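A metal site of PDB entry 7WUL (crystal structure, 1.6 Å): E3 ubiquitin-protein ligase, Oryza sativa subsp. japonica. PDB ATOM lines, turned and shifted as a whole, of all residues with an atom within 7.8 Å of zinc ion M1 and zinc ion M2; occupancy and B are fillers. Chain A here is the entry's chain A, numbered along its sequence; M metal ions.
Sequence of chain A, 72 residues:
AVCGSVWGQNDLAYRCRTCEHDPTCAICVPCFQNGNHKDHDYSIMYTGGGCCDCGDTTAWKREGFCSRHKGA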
ATOM      1  N   ALA A   1      37.111 -15.816 -25.187  1.00  0.00           N
ATOM      2  CA  ALA A   1      37.475 -15.575 -26.583  1.00  0.00           C
ATOM      3  C   ALA A   1      36.301 -15.848 -27.539  1.00  0.00           C
ATOM      4  O   ALA A   1      36.022 -15.032 -28.411  1.00  0.00           O
ATOM      5  CB  ALA A   1      38.688 -16.427 -26.984  1.00  0.00           C
ATOM      6  N   VAL A   2      35.645 -17.001 -27.378  1.00  0.00           N
ATOM      7  CA  VAL A   2      34.548 -17.434 -28.229  1.00  0.00           C
ATOM      8  C   VAL A   2      33.357 -17.713 -27.333  1.00  0.00           C
ATOM      9  O   VAL A   2      33.484 -18.461 -26.351  1.00  0.00           O
ATOM     10  CB  VAL A   2      34.916 -18.682 -29.053  1.00  0.00           C
ATOM     11  CG1 VAL A   2      33.671 -19.296 -29.691  1.00  0.00           C
ATOM     12  CG2 VAL A   2      35.943 -18.338 -30.108  1.00  0.00           C
ATOM     13  N   CYS A   3      32.205 -17.154 -27.689  1.00  0.00           N
ATOM     14  CA  CYS A   3      31.016 -17.283 -26.852  1.00  0.00           C
ATOM     15  C   CYS A   3      30.714 -18.757 -26.579  1.00  0.00           C
ATOM     16  O   CYS A   3      30.554 -19.552 -27.506  1.00  0.00           O
ATOM     17  CB  CYS A   3      29.834 -16.623 -27.559  1.00  0.00           C
ATOM     18  SG  CYS A   3      28.336 -16.697 -26.592  1.00  0.00           S
ATOM     19  N   GLY A   4      30.594 -19.101 -25.310  1.00  0.00           N
ATOM     20  CA  GLY A   4      30.286 -20.488 -25.001  1.00  0.00           C
ATOM     21  C   GLY A   4      28.802 -20.793 -24.890  1.00  0.00           C
ATOM     22  O   GLY A   4      28.429 -21.814 -24.306  1.00  0.00           O
ATOM     23  N   SER A   5      27.937 -19.947 -25.445  1.00  0.00           N
ATOM     24  CA  SER A   5      26.508 -20.114 -25.202  1.00  0.00           C
ATOM     25  C   SER A   5      25.951 -21.272 -26.025  1.00  0.00           C
ATOM     26  O   SER A   5      26.252 -21.427 -27.205  1.00  0.00           O
ATOM     27  CB  SER A   5      25.745 -18.828 -25.506  1.00  0.00           C
ATOM     28  OG  SER A   5      24.433 -18.905 -24.964  1.00  0.00           O
ATOM     29  N   VAL A   6      25.134 -22.089 -25.382  1.00  0.00           N
ATOM     30  CA  VAL A   6      24.466 -23.184 -26.050  1.00  0.00           C
ATOM     31  C   VAL A   6      22.969 -22.948 -25.940  1.00  0.00           C
ATOM     32  O   VAL A   6      22.488 -22.301 -25.006  1.00  0.00           O
ATOM     33  CB  VAL A   6      24.829 -24.555 -25.451  1.00  0.00           C
ATOM     34  CG1 VAL A   6      26.325 -24.780 -25.569  1.00  0.00           C
ATOM     35  CG2 VAL A   6      24.392 -24.618 -24.002  1.00  0.00           C
ATOM     36  N   TRP A   7      22.234 -23.445 -26.933  1.00  0.00           N
ATOM     37  CA  TRP A   7      20.786 -23.344 -26.898  1.00  0.00           C
ATOM     38  C   TRP A   7      20.171 -24.600 -27.495  1.00  0.00           C
ATOM     39  O   TRP A   7      20.834 -25.396 -28.181  1.00  0.00           O
ATOM     40  CB  TRP A   7      20.275 -22.086 -27.627  1.00  0.00           C
ATOM     41  CG  TRP A   7      20.559 -22.060 -29.111  1.00  0.00           C
ATOM     42  CD1 TRP A   7      19.743 -22.514 -30.115  1.00  0.00           C
ATOM     43  CD2 TRP A   7      21.711 -21.501 -29.758  1.00  0.00           C
ATOM     44  NE1 TRP A   7      20.314 -22.281 -31.340  1.00  0.00           N
ATOM     45  CE2 TRP A   7      21.535 -21.684 -31.145  1.00  0.00           C
ATOM     46  CE3 TRP A   7      22.885 -20.890 -29.292  1.00  0.00           C
ATOM     47  CZ2 TRP A   7      22.475 -21.254 -32.079  1.00  0.00           C
ATOM     48  CZ3 TRP A   7      23.810 -20.475 -30.220  1.00  0.00           C
ATOM     49  CH2 TRP A   7      23.615 -20.661 -31.597  1.00  0.00           C
ATOM     50  N   ALA A  26      25.740 -19.855 -36.704  1.00  0.00           N
ATOM     51  CA  ALA A  26      24.695 -19.116 -36.003  1.00  0.00           C
ATOM     52  C   ALA A  26      25.296 -18.485 -34.763  1.00  0.00           C
ATOM     53  O   ALA A  26      26.263 -18.996 -34.187  1.00  0.00           O
ATOM     54  CB  ALA A  26      23.517 -20.016 -35.592  1.00  0.00           C
ATOM     55  N   ILE A  27      24.696 -17.378 -34.337  1.00  0.00           N
ATOM     56  CA  ILE A  27      25.102 -16.757 -33.077  1.00  0.00           C
ATOM     57  C   ILE A  27      23.885 -16.554 -32.188  1.00  0.00           C
ATOM     58  O   ILE A  27      22.741 -16.512 -32.653  1.00  0.00           O
ATOM     59  CB  ILE A  27      25.863 -15.419 -33.280  1.00  0.00           C
ATOM     60  CG1 ILE A  27      24.969 -14.336 -33.914  1.00  0.00           C
ATOM     61  CG2 ILE A  27      27.172 -15.670 -34.069  1.00  0.00           C
ATOM     62  CD1 ILE A  27      25.666 -12.963 -34.009  1.00  0.00           C
ATOM     63  N   CYS A  28      24.136 -16.485 -30.887  1.00  0.00           N
ATOM     64  CA  CYS A  28      23.061 -16.381 -29.906  1.00  0.00           C
ATOM     65  C   CYS A  28      22.416 -14.993 -29.969  1.00  0.00           C
ATOM     66  O   CYS A  28      22.974 -14.044 -30.504  1.00  0.00           O
ATOM     67  CB  CYS A  28      23.579 -16.696 -28.492  1.00  0.00           C
ATOM     68  SG  CYS A  28      24.682 -15.459 -27.755  1.00  0.00           S
ATOM     69  N   VAL A  29      21.195 -14.902 -29.441  1.00  0.00           N
ATOM     70  CA  VAL A  29      20.483 -13.617 -29.489  1.00  0.00           C
ATOM     71  C   VAL A  29      21.295 -12.502 -28.845  1.00  0.00           C
ATOM     72  O   VAL A  29      21.444 -11.437 -29.461  1.00  0.00           O
ATOM     73  CB  VAL A  29      19.080 -13.766 -28.874  1.00  0.00           C
ATOM     74  CG1 VAL A  29      18.470 -12.374 -28.670  1.00  0.00           C
ATOM     75  CG2 VAL A  29      18.199 -14.615 -29.758  1.00  0.00           C
ATOM     76  N   PRO A  30      21.865 -12.663 -27.640  1.00  0.00           N
ATOM     77  CA  PRO A  30      22.610 -11.532 -27.082  1.00  0.00           C
ATOM     78  C   PRO A  30      23.840 -11.141 -27.891  1.00  0.00           C
ATOM     79  O   PRO A  30      24.152  -9.941 -27.986  1.00  0.00           O
ATOM     80  CB  PRO A  30      22.981 -12.005 -25.666  1.00  0.00           C
ATOM     81  CG  PRO A  30      22.093 -13.123 -25.379  1.00  0.00           C
ATOM     82  CD  PRO A  30      21.581 -13.702 -26.648  1.00  0.00           C
ATOM     83  N   CYS A  31      24.543 -12.092 -28.509  1.00  0.00           N
ATOM     84  CA  CYS A  31      25.686 -11.721 -29.341  1.00  0.00           C
ATOM     85  C   CYS A  31      25.220 -10.977 -30.584  1.00  0.00           C
ATOM     86  O   CYS A  31      25.899 -10.045 -31.030  1.00  0.00           O
ATOM     87  CB  CYS A  31      26.492 -12.940 -29.741  1.00  0.00           C
ATOM     88  SG  CYS A  31      27.537 -13.523 -28.380  1.00  0.00           S
ATOM     89  N   PHE A  32      24.075 -11.352 -31.153  1.00  0.00           N
ATOM     90  CA  PHE A  32      23.578 -10.566 -32.282  1.00  0.00           C
ATOM     91  C   PHE A  32      23.244  -9.134 -31.854  1.00  0.00           C
ATOM     92  O   PHE A  32      23.627  -8.158 -32.527  1.00  0.00           O
ATOM     93  CB  PHE A  32      22.340 -11.237 -32.915  1.00  0.00           C
ATOM     94  CG  PHE A  32      21.819 -10.473 -34.084  1.00  0.00           C
ATOM     95  CD1 PHE A  32      20.871  -9.464 -33.937  1.00  0.00           C
ATOM     96  CD2 PHE A  32      22.354 -10.708 -35.343  1.00  0.00           C
ATOM     97  CE1 PHE A  32      20.435  -8.724 -35.044  1.00  0.00           C
ATOM     98  CE2 PHE A  32      21.917  -9.978 -36.428  1.00  0.00           C
ATOM     99  CZ  PHE A  32      20.967  -8.990 -36.273  1.00  0.00           C
ATOM    100  N   ASN A  34      24.353  -7.320 -29.456  1.00  0.00           N
ATOM    101  CA  ASN A  34      25.511  -6.529 -29.091  1.00  0.00           C
ATOM    102  C   ASN A  34      26.516  -6.379 -30.218  1.00  0.00           C
ATOM    103  O   ASN A  34      27.610  -5.841 -30.009  1.00  0.00           O
ATOM    104  CB  ASN A  34      26.175  -7.123 -27.848  1.00  0.00           C
ATOM    105  CG  ASN A  34      25.373  -6.839 -26.593  1.00  0.00           C
ATOM    106  OD1 ASN A  34      24.702  -5.808 -26.502  1.00  0.00           O
ATOM    107  ND2 ASN A  34      25.424  -7.761 -25.644  1.00  0.00           N
ATOM    108  N   GLY A  35      26.152  -6.823 -31.423  1.00  0.00           N
ATOM    109  CA  GLY A  35      26.951  -6.636 -32.607  1.00  0.00           C
ATOM    110  C   GLY A  35      26.281  -5.709 -33.620  1.00  0.00           C
ATOM    111  O   GLY A  35      25.200  -5.164 -33.412  1.00  0.00           O
ATOM    112  N   CYS A  51      25.613 -24.095 -30.785  1.00  0.00           N
ATOM    113  CA  CYS A  51      26.615 -23.432 -29.973  1.00  0.00           C
ATOM    114  C   CYS A  51      27.048 -22.165 -30.677  1.00  0.00           C
ATOM    115  O   CYS A  51      27.288 -22.178 -31.892  1.00  0.00           O
ATOM    116  CB  CYS A  51      27.849 -24.321 -29.762  1.00  0.00           C
ATOM    117  SG  CYS A  51      27.524 -25.868 -28.919  1.00  0.00           S
ATOM    118  N   CYS A  52      27.170 -21.073 -29.928  1.00  0.00           N
ATOM    119  CA  CYS A  52      27.372 -19.771 -30.542  1.00  0.00           C
ATOM    120  C   CYS A  52      28.733 -19.700 -31.247  1.00  0.00           C
ATOM    121  O   CYS A  52      29.759 -20.148 -30.714  1.00  0.00           O
ATOM    122  CB  CYS A  52      27.297 -18.683 -29.470  1.00  0.00           C
ATOM    123  SG  CYS A  52      27.330 -17.035 -30.182  1.00  0.00           S
ATOM    124  N   ASP A  53      28.746 -19.111 -32.437  1.00  0.00           N
ATOM    125  CA  ASP A  53      29.968 -18.932 -33.198  1.00  0.00           C
ATOM    126  C   ASP A  53      30.621 -17.568 -33.005  1.00  0.00           C
ATOM    127  O   ASP A  53      31.650 -17.294 -33.636  1.00  0.00           O
ATOM    128  CB  ASP A  53      29.697 -19.141 -34.689  1.00  0.00           C
ATOM    129  CG  ASP A  53      29.349 -20.579 -35.026  1.00  0.00           C
ATOM    130  OD1 ASP A  53      29.902 -21.498 -34.383  1.00  0.00           O
ATOM    131  OD2 ASP A  53      28.502 -20.775 -35.924  1.00  0.00           O
ATOM    132  N   CYS A  54      30.059 -16.717 -32.151  1.00  0.00           N
ATOM    133  CA  CYS A  54      30.588 -15.369 -32.018  1.00  0.00           C
ATOM    134  C   CYS A  54      31.991 -15.384 -31.417  1.00  0.00           C
ATOM    135  O   CYS A  54      32.208 -15.943 -30.335  1.00  0.00           O
ATOM    136  CB  CYS A  54      29.654 -14.534 -31.156  1.00  0.00           C
ATOM    137  SG  CYS A  54      30.135 -12.814 -30.998  1.00  0.00           S
ATOM    138  N   GLY A  55      32.929 -14.763 -32.110  1.00  0.00           N
ATOM    139  CA  GLY A  55      34.324 -14.751 -31.700  1.00  0.00           C
ATOM    140  C   GLY A  55      35.199 -15.757 -32.389  1.00  0.00           C
ATOM    141  O   GLY A  55      36.431 -15.701 -32.252  1.00  0.00           O
ATOM    142  N   GLY A  64      31.477  -9.143 -37.668  1.00  0.00           N
ATOM    143  CA  GLY A  64      30.223  -9.544 -37.087  1.00  0.00           C
ATOM    144  C   GLY A  64      30.308 -10.023 -35.654  1.00  0.00           C
ATOM    145  O   GLY A  64      29.305 -10.531 -35.132  1.00  0.00           O
ATOM    146  N   PHE A  65      31.463  -9.911 -35.001  1.00  0.00           N
ATOM    147  CA  PHE A  65      31.584 -10.254 -33.591  1.00  0.00           C
ATOM    148  C   PHE A  65      30.900  -9.195 -32.731  1.00  0.00           C
ATOM    149  O   PHE A  65      30.961  -7.993 -33.020  1.00  0.00           O
ATOM    150  CB  PHE A  65      33.056 -10.348 -33.160  1.00  0.00           C
ATOM    151  CG  PHE A  65      33.842 -11.460 -33.809  1.00  0.00           C
ATOM    152  CD1 PHE A  65      33.223 -12.455 -34.553  1.00  0.00           C
ATOM    153  CD2 PHE A  65      35.223 -11.526 -33.613  1.00  0.00           C
ATOM    154  CE1 PHE A  65      33.978 -13.470 -35.134  1.00  0.00           C
ATOM    155  CE2 PHE A  65      35.972 -12.549 -34.181  1.00  0.00           C
ATOM    156  CZ  PHE A  65      35.349 -13.521 -34.942  1.00  0.00           C
ATOM    157  N   CYS A  66      30.281  -9.634 -31.648  1.00  0.00           N
ATOM    158  CA  CYS A  66      29.712  -8.663 -30.724  1.00  0.00           C
ATOM    159  C   CYS A  66      30.838  -7.972 -29.934  1.00  0.00           C
ATOM    160  O   CYS A  66      32.001  -8.380 -29.954  1.00  0.00           O
ATOM    161  CB  CYS A  66      28.712  -9.317 -29.774  1.00  0.00           C
ATOM    162  SG  CYS A  66      29.426 -10.137 -28.318  1.00  0.00           S
ATOM    163  N   SER A  67      30.453  -6.899 -29.240  1.00  0.00           N
ATOM    164  CA  SER A  67      31.434  -6.098 -28.514  1.00  0.00           C
ATOM    165  C   SER A  67      32.155  -6.884 -27.413  1.00  0.00           C
ATOM    166  O   SER A  67      33.248  -6.476 -27.008  1.00  0.00           O
ATOM    167  CB  SER A  67      30.743  -4.872 -27.918  1.00  0.00           C
ATOM    168  OG  SER A  67      29.601  -5.243 -27.158  1.00  0.00           O
ATOM    169  N   ARG A  68      31.597  -8.003 -26.967  1.00  0.00           N
ATOM    170  CA  ARG A  68      32.110  -8.764 -25.829  1.00  0.00           C
ATOM    171  C   ARG A  68      33.031  -9.909 -26.233  1.00  0.00           C
ATOM    172  O   ARG A  68      33.722 -10.445 -25.363  1.00  0.00           O
ATOM    173  CB  ARG A  68      30.940  -9.307 -24.999  1.00  0.00           C
ATOM    174  CG  ARG A  68      30.095  -8.171 -24.428  1.00  0.00           C
ATOM    175  CD  ARG A  68      28.966  -8.582 -23.483  1.00  0.00           C
ATOM    176  NE  ARG A  68      29.438  -9.379 -22.365  1.00  0.00           N
ATOM    177  CZ  ARG A  68      29.352 -10.698 -22.305  1.00  0.00           C
ATOM    178  NH1 ARG A  68      28.709 -11.381 -23.232  1.00  0.00           N
ATOM    179  NH2 ARG A  68      29.924 -11.340 -21.293  1.00  0.00           N
ATOM    180  N   HIS A  69      33.031 -10.312 -27.507  1.00  0.00           N
ATOM    181  CA  HIS A  69      33.953 -11.317 -28.020  1.00  0.00           C
ATOM    182  C   HIS A  69      34.754 -10.766 -29.198  1.00  0.00           C
ATOM    183  O   HIS A  69      35.185 -11.523 -30.069  1.00  0.00           O
ATOM    184  CB  HIS A  69      33.227 -12.619 -28.369  1.00  0.00           C
ATOM    185  CG  HIS A  69      32.296 -13.086 -27.294  1.00  0.00           C
ATOM    186  ND1 HIS A  69      30.916 -13.033 -27.409  1.00  0.00           N
ATOM    187  CD2 HIS A  69      32.554 -13.598 -26.070  1.00  0.00           C
ATOM    188  CE1 HIS A  69      30.375 -13.491 -26.295  1.00  0.00           C
ATOM    189  NE2 HIS A  69      31.348 -13.846 -25.468  1.00  0.00           N
ATOM    190  N   LYS A  70      34.973  -9.456 -29.209  1.00  0.00           N
ATOM    191  CA  LYS A  70      35.806  -8.812 -30.228  1.00  0.00           C
ATOM    192  C   LYS A  70      37.098  -8.323 -29.601  1.00  0.00           C
ATOM    193  O   LYS A  70      37.847  -9.114 -29.021  1.00  0.00           O
ATOM    194  CB  LYS A  70      35.045  -7.661 -30.890  1.00  0.00           C
ATOM    195  CG  LYS A  70      35.234  -6.306 -30.225  1.00  0.00           C
ATOM    196  CD  LYS A  70      34.367  -5.253 -30.931  1.00  0.00           C
ATOM    197  CE  LYS A  70      34.447  -3.887 -30.244  1.00  0.00           C
ATOM    198  NZ  LYS A  70      33.355  -2.975 -30.704  1.00  0.00           N
HETATM  199 ZN    ZN M   1      26.938 -15.824 -28.228  1.00  0.00          ZN
HETATM  200 ZN    ZN M   2      29.552 -12.368 -28.831  1.00  0.00          ZN
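The backbone carbonyl oxygen of Cys 54 lies within hydrogen-bond range of the backbone NH of Cys 3 (2.9 Å).
N of Cys 54 lies close to SG of Cys 52, at 3.4 Å.
N of Arg 68 lies close to SG of Cys 66.
The side-chain sulfur of Cys 3 lies close to the backbone NH of Ser 5 (3.5 Å).
The backbone NH of Cys 52 is in hydrogen-bond range of the backbone carbonyl oxygen of Ser 5, 2.9 Å away.
Four residues have an atom within 4 Å of zinc ion M1: Cys 3, Cys 28, Cys 31 and Cys 52.
Of the 28 residues printed, 4 come within 4 Å of zinc ion M2.
Zinc ion M1 is bound by SG of Cys 3 (2.3 Å), SG of Cys 52 (2.3 Å), SG of Cys 28 (2.3 Å) and SG of Cys 31 (2.4 Å).
Zinc ion M1 has four donor atoms within binding distance.
Zinc ion M2 is bound by a ring nitrogen (ND1) of His 69 (2.1 Å), the side-chain sulfur of Cys 54 (2.3 Å), the side-chain sulfur of Cys 66 (2.3 Å) and the side-chain sulfur of Cys 31 (2.4 Å).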
